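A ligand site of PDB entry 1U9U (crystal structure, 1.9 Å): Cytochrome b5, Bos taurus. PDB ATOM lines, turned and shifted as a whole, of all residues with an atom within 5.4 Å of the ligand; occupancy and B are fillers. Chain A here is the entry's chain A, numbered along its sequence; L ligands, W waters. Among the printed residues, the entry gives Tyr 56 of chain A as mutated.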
ATOM      1  N   LEU A  21      19.602 -20.237  21.295  1.00  0.00           N
ATOM      2  CA  LEU A  21      20.125 -21.480  20.785  1.00  0.00           C
ATOM      3  C   LEU A  21      19.032 -22.193  20.020  1.00  0.00           C
ATOM      4  O   LEU A  21      17.851 -21.893  20.167  1.00  0.00           O
ATOM      5  CB  LEU A  21      20.724 -22.348  21.883  1.00  0.00           C
ATOM      6  CG  LEU A  21      19.982 -22.812  23.115  1.00  0.00           C
ATOM      7  CD1 LEU A  21      18.945 -23.861  22.750  1.00  0.00           C
ATOM      8  CD2 LEU A  21      20.996 -23.398  24.087  1.00  0.00           C
ATOM      9  N   LEU A  23      17.140 -25.815  18.870  1.00  0.00           N
ATOM     10  CA  LEU A  23      16.841 -27.177  19.274  1.00  0.00           C
ATOM     11  C   LEU A  23      15.760 -27.674  18.324  1.00  0.00           C
ATOM     12  O   LEU A  23      14.682 -27.082  18.265  1.00  0.00           O
ATOM     13  CB  LEU A  23      16.322 -27.240  20.719  1.00  0.00           C
ATOM     14  CG  LEU A  23      17.253 -26.813  21.849  1.00  0.00           C
ATOM     15  CD1 LEU A  23      16.518 -26.915  23.175  1.00  0.00           C
ATOM     16  CD2 LEU A  23      18.489 -27.705  21.867  1.00  0.00           C
ATOM     17  N   TYR A  28      15.260 -20.759  20.625  1.00  0.00           N
ATOM     18  CA  TYR A  28      14.897 -20.489  22.008  1.00  0.00           C
ATOM     19  C   TYR A  28      15.690 -19.326  22.578  1.00  0.00           C
ATOM     20  O   TYR A  28      16.886 -19.217  22.331  1.00  0.00           O
ATOM     21  CB  TYR A  28      15.165 -21.712  22.878  1.00  0.00           C
ATOM     22  CG  TYR A  28      14.391 -22.949  22.480  1.00  0.00           C
ATOM     23  CD1 TYR A  28      14.661 -23.610  21.286  1.00  0.00           C
ATOM     24  CD2 TYR A  28      13.390 -23.463  23.313  1.00  0.00           C
ATOM     25  CE1 TYR A  28      13.945 -24.743  20.917  1.00  0.00           C
ATOM     26  CE2 TYR A  28      12.670 -24.597  22.958  1.00  0.00           C
ATOM     27  CZ  TYR A  28      12.964 -25.230  21.758  1.00  0.00           C
ATOM     28  OH  TYR A  28      12.272 -26.364  21.412  1.00  0.00           O
ATOM     29  N   LEU A  30      16.995 -18.205  25.823  1.00  0.00           N
ATOM     30  CA  LEU A  30      17.204 -18.668  27.194  1.00  0.00           C
ATOM     31  C   LEU A  30      17.834 -17.657  28.114  1.00  0.00           C
ATOM     32  O   LEU A  30      18.217 -17.983  29.234  1.00  0.00           O
ATOM     33  CB  LEU A  30      18.051 -19.939  27.171  1.00  0.00           C
ATOM     34  CG  LEU A  30      17.483 -21.069  26.308  1.00  0.00           C
ATOM     35  CD1 LEU A  30      18.374 -22.300  26.456  1.00  0.00           C
ATOM     36  CD2 LEU A  30      16.058 -21.388  26.735  1.00  0.00           C
ATOM     37  N   PHE A  33      16.624 -17.762  31.582  1.00  0.00           N
ATOM     38  CA  PHE A  33      16.564 -19.109  32.132  1.00  0.00           C
ATOM     39  C   PHE A  33      17.933 -19.605  32.624  1.00  0.00           C
ATOM     40  O   PHE A  33      18.017 -20.565  33.408  1.00  0.00           O
ATOM     41  CB  PHE A  33      16.036 -20.058  31.054  1.00  0.00           C
ATOM     42  CG  PHE A  33      15.869 -21.475  31.502  1.00  0.00           C
ATOM     43  CD1 PHE A  33      16.540 -22.500  30.840  1.00  0.00           C
ATOM     44  CD2 PHE A  33      15.039 -21.793  32.559  1.00  0.00           C
ATOM     45  CE1 PHE A  33      16.384 -23.822  31.230  1.00  0.00           C
ATOM     46  CE2 PHE A  33      14.888 -23.116  32.965  1.00  0.00           C
ATOM     47  CZ  PHE A  33      15.559 -24.127  32.304  1.00  0.00           C
ATOM     48  N   HIS A  37      18.276 -22.917  35.210  1.00  0.00           N
ATOM     49  CA  HIS A  37      18.558 -24.222  34.624  1.00  0.00           C
ATOM     50  C   HIS A  37      19.209 -25.191  35.607  1.00  0.00           C
ATOM     51  O   HIS A  37      20.324 -24.950  36.066  1.00  0.00           O
ATOM     52  CB  HIS A  37      19.479 -24.039  33.424  1.00  0.00           C
ATOM     53  CG  HIS A  37      19.742 -25.299  32.664  1.00  0.00           C
ATOM     54  ND1 HIS A  37      20.990 -25.675  32.216  1.00  0.00           N
ATOM     55  CD2 HIS A  37      18.890 -26.270  32.248  1.00  0.00           C
ATOM     56  CE1 HIS A  37      20.854 -26.818  31.549  1.00  0.00           C
ATOM     57  NE2 HIS A  37      19.598 -27.223  31.542  1.00  0.00           N
ATOM     58  N   PRO A  38      18.527 -26.292  35.931  1.00  0.00           N
ATOM     59  CA  PRO A  38      19.104 -27.272  36.877  1.00  0.00           C
ATOM     60  C   PRO A  38      20.466 -27.771  36.420  1.00  0.00           C
ATOM     61  O   PRO A  38      21.281 -28.202  37.236  1.00  0.00           O
ATOM     62  CB  PRO A  38      18.050 -28.363  36.911  1.00  0.00           C
ATOM     63  CG  PRO A  38      16.769 -27.615  36.680  1.00  0.00           C
ATOM     64  CD  PRO A  38      17.161 -26.682  35.559  1.00  0.00           C
ATOM     65  N   GLY A  39      20.710 -27.731  35.120  1.00  0.00           N
ATOM     66  CA  GLY A  39      21.981 -28.202  34.585  1.00  0.00           C
ATOM     67  C   GLY A  39      23.074 -27.151  34.627  1.00  0.00           C
ATOM     68  O   GLY A  39      24.199 -27.419  34.184  1.00  0.00           O
ATOM     69  N   VAL A  43      26.734 -24.786  30.732  1.00  0.00           N
ATOM     70  CA  VAL A  43      26.428 -25.710  29.647  1.00  0.00           C
ATOM     71  C   VAL A  43      25.567 -25.050  28.563  1.00  0.00           C
ATOM     72  O   VAL A  43      25.619 -25.446  27.398  1.00  0.00           O
ATOM     73  CB  VAL A  43      25.703 -26.965  30.202  1.00  0.00           C
ATOM     74  CG1 VAL A  43      24.377 -26.577  30.841  1.00  0.00           C
ATOM     75  CG2 VAL A  43      25.477 -27.968  29.085  1.00  0.00           C
ATOM     76  N   LEU A  44      24.801 -24.035  28.944  1.00  0.00           N
ATOM     77  CA  LEU A  44      23.958 -23.332  27.978  1.00  0.00           C
ATOM     78  C   LEU A  44      24.757 -22.287  27.221  1.00  0.00           C
ATOM     79  O   LEU A  44      24.688 -22.195  26.000  1.00  0.00           O
ATOM     80  CB  LEU A  44      22.781 -22.676  28.713  1.00  0.00           C
ATOM     81  CG  LEU A  44      21.845 -23.599  29.487  1.00  0.00           C
ATOM     82  CD1 LEU A  44      20.718 -22.782  30.112  1.00  0.00           C
ATOM     83  CD2 LEU A  44      21.269 -24.661  28.558  1.00  0.00           C
ATOM     84  N   GLN A  47      26.794 -23.396  24.261  1.00  0.00           N
ATOM     85  CA  GLN A  47      26.084 -23.730  23.032  1.00  0.00           C
ATOM     86  C   GLN A  47      25.416 -22.525  22.380  1.00  0.00           C
ATOM     87  O   GLN A  47      24.955 -22.599  21.225  1.00  0.00           O
ATOM     88  CB  GLN A  47      25.016 -24.786  23.323  1.00  0.00           C
ATOM     89  CG  GLN A  47      25.562 -26.071  23.919  1.00  0.00           C
ATOM     90  CD  GLN A  47      26.506 -26.796  22.977  1.00  0.00           C
ATOM     91  OE1 GLN A  47      26.162 -27.078  21.824  1.00  0.00           O
ATOM     92  NE2 GLN A  47      27.694 -27.118  23.467  1.00  0.00           N
ATOM     93  N   ALA A  52      22.168 -26.868  19.454  1.00  0.00           N
ATOM     94  CA  ALA A  52      22.575 -27.718  20.570  1.00  0.00           C
ATOM     95  C   ALA A  52      21.664 -28.932  20.701  1.00  0.00           C
ATOM     96  O   ALA A  52      21.605 -29.557  21.761  1.00  0.00           O
ATOM     97  CB  ALA A  52      22.539 -26.912  21.871  1.00  0.00           C
ATOM     98  N   ASN A  55      23.466 -32.342  21.961  1.00  0.00           N
ATOM     99  CA  ASN A  55      23.851 -32.287  23.367  1.00  0.00           C
ATOM    100  C   ASN A  55      22.621 -32.304  24.259  1.00  0.00           C
ATOM    101  O   ASN A  55      22.656 -32.835  25.367  1.00  0.00           O
ATOM    102  CB  ASN A  55      24.660 -31.024  23.651  1.00  0.00           C
ATOM    103  CG  ASN A  55      25.881 -30.908  22.761  1.00  0.00           C
ATOM    104  OD1 ASN A  55      25.771 -30.682  21.556  1.00  0.00           O
ATOM    105  ND2 ASN A  55      27.054 -31.065  23.359  1.00  0.00           N
ATOM    106  N   TYR A  56      21.549 -31.722  23.765  1.00  0.00           N
ATOM    107  CA  TYR A  56      20.297 -31.652  24.500  1.00  0.00           C
ATOM    108  C   TYR A  56      19.664 -33.034  24.625  1.00  0.00           C
ATOM    109  O   TYR A  56      19.199 -33.425  25.708  1.00  0.00           O
ATOM    110  CB  TYR A  56      19.330 -30.726  23.767  1.00  0.00           C
ATOM    111  CG  TYR A  56      17.967 -30.612  24.389  1.00  0.00           C
ATOM    112  CD1 TYR A  56      17.771 -29.859  25.558  1.00  0.00           C
ATOM    113  CD2 TYR A  56      16.862 -31.199  23.783  1.00  0.00           C
ATOM    114  CE1 TYR A  56      16.504 -29.714  26.107  1.00  0.00           C
ATOM    115  CE2 TYR A  56      15.588 -31.061  24.322  1.00  0.00           C
ATOM    116  CZ  TYR A  56      15.417 -30.314  25.476  1.00  0.00           C
ATOM    117  OH  TYR A  56      14.148 -30.152  25.967  1.00  0.00           O
ATOM    118  N   VAL A  59      21.656 -35.718  26.874  1.00  0.00           N
ATOM    119  CA  VAL A  59      21.421 -35.744  28.318  1.00  0.00           C
ATOM    120  C   VAL A  59      20.060 -36.356  28.631  1.00  0.00           C
ATOM    121  O   VAL A  59      19.792 -36.740  29.758  1.00  0.00           O
ATOM    122  CB  VAL A  59      21.473 -34.327  28.914  1.00  0.00           C
ATOM    123  CG1 VAL A  59      22.878 -33.762  28.797  1.00  0.00           C
ATOM    124  CG2 VAL A  59      20.499 -33.451  28.198  1.00  0.00           C
ATOM    125  N   GLY A  60      19.203 -36.437  27.614  1.00  0.00           N
ATOM    126  CA  GLY A  60      17.874 -37.014  27.791  1.00  0.00           C
ATOM    127  C   GLY A  60      16.975 -36.307  28.790  1.00  0.00           C
ATOM    128  O   GLY A  60      16.649 -36.862  29.840  1.00  0.00           O
ATOM    129  N   HIS A  61      16.574 -35.083  28.471  1.00  0.00           N
ATOM    130  CA  HIS A  61      15.693 -34.313  29.346  1.00  0.00           C
ATOM    131  C   HIS A  61      14.369 -35.001  29.600  1.00  0.00           C
ATOM    132  O   HIS A  61      13.866 -35.722  28.747  1.00  0.00           O
ATOM    133  CB  HIS A  61      15.450 -32.930  28.764  1.00  0.00           C
ATOM    134  CG  HIS A  61      16.596 -31.993  28.928  1.00  0.00           C
ATOM    135  ND1 HIS A  61      17.754 -32.061  28.194  1.00  0.00           N
ATOM    136  CD2 HIS A  61      16.790 -30.999  29.834  1.00  0.00           C
ATOM    137  CE1 HIS A  61      18.599 -31.121  28.665  1.00  0.00           C
ATOM    138  NE2 HIS A  61      18.045 -30.456  29.656  1.00  0.00           N
ATOM    139  N   SER A  62      13.814 -34.765  30.782  1.00  0.00           N
ATOM    140  CA  SER A  62      12.540 -35.376  31.159  1.00  0.00           C
ATOM    141  C   SER A  62      11.380 -34.702  30.443  1.00  0.00           C
ATOM    142  O   SER A  62      11.538 -33.663  29.803  1.00  0.00           O
ATOM    143  CB  SER A  62      12.329 -35.279  32.675  1.00  0.00           C
ATOM    144  OG  SER A  62      12.335 -33.922  33.107  1.00  0.00           O
ATOM    145  N   ALA A  65      10.720 -31.122  31.532  1.00  0.00           N
ATOM    146  CA  ALA A  65      11.703 -30.179  31.017  1.00  0.00           C
ATOM    147  C   ALA A  65      11.344 -29.765  29.584  1.00  0.00           C
ATOM    148  O   ALA A  65      11.466 -28.599  29.220  1.00  0.00           O
ATOM    149  CB  ALA A  65      13.095 -30.804  31.036  1.00  0.00           C
ATOM    150  N   LEU A  68       8.385 -27.435  29.577  1.00  0.00           N
ATOM    151  CA  LEU A  68       8.797 -26.106  29.974  1.00  0.00           C
ATOM    152  C   LEU A  68       9.558 -25.360  28.888  1.00  0.00           C
ATOM    153  O   LEU A  68       9.425 -24.152  28.752  1.00  0.00           O
ATOM    154  CB  LEU A  68       9.671 -26.174  31.232  1.00  0.00           C
ATOM    155  CG  LEU A  68      10.315 -24.851  31.655  1.00  0.00           C
ATOM    156  CD1 LEU A  68       9.252 -23.834  31.984  1.00  0.00           C
ATOM    157  CD2 LEU A  68      11.236 -25.093  32.838  1.00  0.00           C
ATOM    158  N   SER A  69      10.349 -26.091  28.106  1.00  0.00           N
ATOM    159  CA  SER A  69      11.150 -25.481  27.047  1.00  0.00           C
ATOM    160  C   SER A  69      10.285 -24.699  26.057  1.00  0.00           C
ATOM    161  O   SER A  69      10.705 -23.679  25.517  1.00  0.00           O
ATOM    162  CB  SER A  69      11.951 -26.540  26.297  1.00  0.00           C
ATOM    163  OG  SER A  69      11.113 -27.370  25.500  1.00  0.00           O
ATOM    164  N   PHE A  72       9.959 -20.856  25.994  1.00  0.00           N
ATOM    165  CA  PHE A  72      11.088 -20.040  25.540  1.00  0.00           C
ATOM    166  C   PHE A  72      11.266 -19.958  24.015  1.00  0.00           C
ATOM    167  O   PHE A  72      12.209 -19.334  23.525  1.00  0.00           O
ATOM    168  CB  PHE A  72      12.381 -20.549  26.178  1.00  0.00           C
ATOM    169  CG  PHE A  72      12.358 -20.542  27.687  1.00  0.00           C
ATOM    170  CD1 PHE A  72      12.225 -19.346  28.387  1.00  0.00           C
ATOM    171  CD2 PHE A  72      12.453 -21.739  28.403  1.00  0.00           C
ATOM    172  CE1 PHE A  72      12.170 -19.338  29.790  1.00  0.00           C
ATOM    173  CE2 PHE A  72      12.400 -21.738  29.799  1.00  0.00           C
ATOM    174  CZ  PHE A  72      12.260 -20.534  30.490  1.00  0.00           C
HETATM  175  C1  LIG L   1      19.063 -30.780  33.399  1.00  0.00           C
HETATM  176  C2  LIG L   1      15.557 -27.969  31.580  1.00  0.00           C
HETATM  177  C3  LIG L   1      18.336 -27.097  27.751  1.00  0.00           C
HETATM  178  C4  LIG L   1      21.968 -29.685  29.701  1.00  0.00           C
HETATM  179  C5  LIG L   1      17.828 -30.167  33.168  1.00  0.00           C
HETATM  180  C6  LIG L   1      16.689 -30.340  34.021  1.00  0.00           C
HETATM  181  C7  LIG L   1      15.731 -29.479  33.561  1.00  0.00           C
HETATM  182  C8  LIG L   1      16.292 -28.817  32.403  1.00  0.00           C
HETATM  183  C9  LIG L   1      14.334 -29.246  34.105  1.00  0.00           C
HETATM  184  C10 LIG L   1      16.562 -31.310  35.192  1.00  0.00           C
HETATM  185  C11 LIG L   1      16.505 -32.757  34.748  1.00  0.00           C
HETATM  186  C12 LIG L   1      15.345 -33.034  33.807  1.00  0.00           C
HETATM  187  O1  LIG L   1      14.198 -32.719  34.187  1.00  0.00           O
HETATM  188  O2  LIG L   1      15.584 -33.557  32.700  1.00  0.00           O
HETATM  189  C13 LIG L   1      16.037 -27.473  30.389  1.00  0.00           C
HETATM  190  C14 LIG L   1      15.253 -26.654  29.483  1.00  0.00           C
HETATM  191  C15 LIG L   1      16.048 -26.371  28.436  1.00  0.00           C
HETATM  192  C16 LIG L   1      17.294 -27.069  28.651  1.00  0.00           C
HETATM  193  C17 LIG L   1      13.815 -26.188  29.672  1.00  0.00           C
HETATM  194  C18 LIG L   1      15.750 -25.418  27.462  1.00  0.00           C
HETATM  195  C19 LIG L   1      15.358 -25.755  26.181  1.00  0.00           C
HETATM  196  C20 LIG L   1      19.541 -27.770  27.933  1.00  0.00           C
HETATM  197  C21 LIG L   1      20.607 -27.780  26.953  1.00  0.00           C
HETATM  198  C22 LIG L   1      21.652 -28.449  27.494  1.00  0.00           C
HETATM  199  C23 LIG L   1      21.206 -28.890  28.823  1.00  0.00           C
HETATM  200  C24 LIG L   1      20.545 -27.127  25.570  1.00  0.00           C
HETATM  201  C25 LIG L   1      22.942 -28.633  27.001  1.00  0.00           C
HETATM  202  C26 LIG L   1      23.483 -28.305  25.761  1.00  0.00           C
HETATM  203  C27 LIG L   1      21.501 -30.161  30.919  1.00  0.00           C
HETATM  204  C28 LIG L   1      22.275 -30.960  31.860  1.00  0.00           C
HETATM  205  C29 LIG L   1      21.445 -31.269  32.881  1.00  0.00           C
HETATM  206  C30 LIG L   1      20.176 -30.638  32.596  1.00  0.00           C
HETATM  207  C31 LIG L   1      23.733 -31.375  31.754  1.00  0.00           C
HETATM  208  C32 LIG L   1      21.785 -32.118  34.117  1.00  0.00           C
HETATM  209  C33 LIG L   1      21.629 -33.599  33.819  1.00  0.00           C
HETATM  210  C34 LIG L   1      21.971 -34.474  35.009  1.00  0.00           C
HETATM  211  O3  LIG L   1      21.891 -35.718  34.872  1.00  0.00           O
HETATM  212  O4  LIG L   1      22.306 -33.932  36.084  1.00  0.00           O
HETATM  213  N1  LIG L   1      17.574 -29.268  32.146  1.00  0.00           N
HETATM  214  N2  LIG L   1      17.303 -27.732  29.863  1.00  0.00           N
HETATM  215  N3  LIG L   1      19.902 -28.487  29.079  1.00  0.00           N
HETATM  216  N4  LIG L   1      20.226 -29.935  31.404  1.00  0.00           N
HETATM  217 FE1  LIG L   1      18.773 -28.855  30.635  1.00  0.00          FE
HETATM  218  O   HOH W   1      13.465 -32.680  36.918  1.00  0.00           O
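Merely in contact with the ligand: Leu 23 (3.4 Å), Phe 33 (3.5 Å), Pro 38 (3.7 Å), Gly 39 (3.5 Å), Val 43 (3.3 Å), Leu 44 (3.6 Å), Gln 47 (3.6 Å), Asn 55 (3.6 Å), Tyr 56 (3.6 Å), Val 59 (3.9 Å), Ala 65 (3.4 Å) and Ser 69 (3.5 Å).
Hydrophobic or aromatic side chains that line the ligand: Leu 23, Phe 33, His 37, Pro 38, Val 43, Leu 44, Tyr 56, Val 59, His 61 and Ala 65.
15 residues have an atom within 4 Å of the ligand: Leu 23, Phe 33, His 37, Pro 38, Gly 39, Val 43, Leu 44, Gln 47, Asn 55, Tyr 56, Val 59, His 61, Ser 62, Ala 65 and Ser 69.
The nearest printed residue that does not touch the ligand is Leu 21 (4.04 Å).
A ring nitrogen (NE2) of His 61 is bound to an iron atom (FE1) of the ligand (2.0 Å).
A ring nitrogen (NE2) of His 37 is bound to an iron atom (FE1) of the ligand (2.0 Å).
The backbone NH (N) of Ser 62 sits at hydrogen-bond distance from an oxygen (O2) of the ligand, 2.9 Å away.
An oxygen (O1) of the ligand lies within hydrogen-bond range of the side-chain hydroxyl (OG) of Ser 62 (2.5 Å).
ND1 of His 61 is in hydrogen-bond range of O of Tyr 56.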
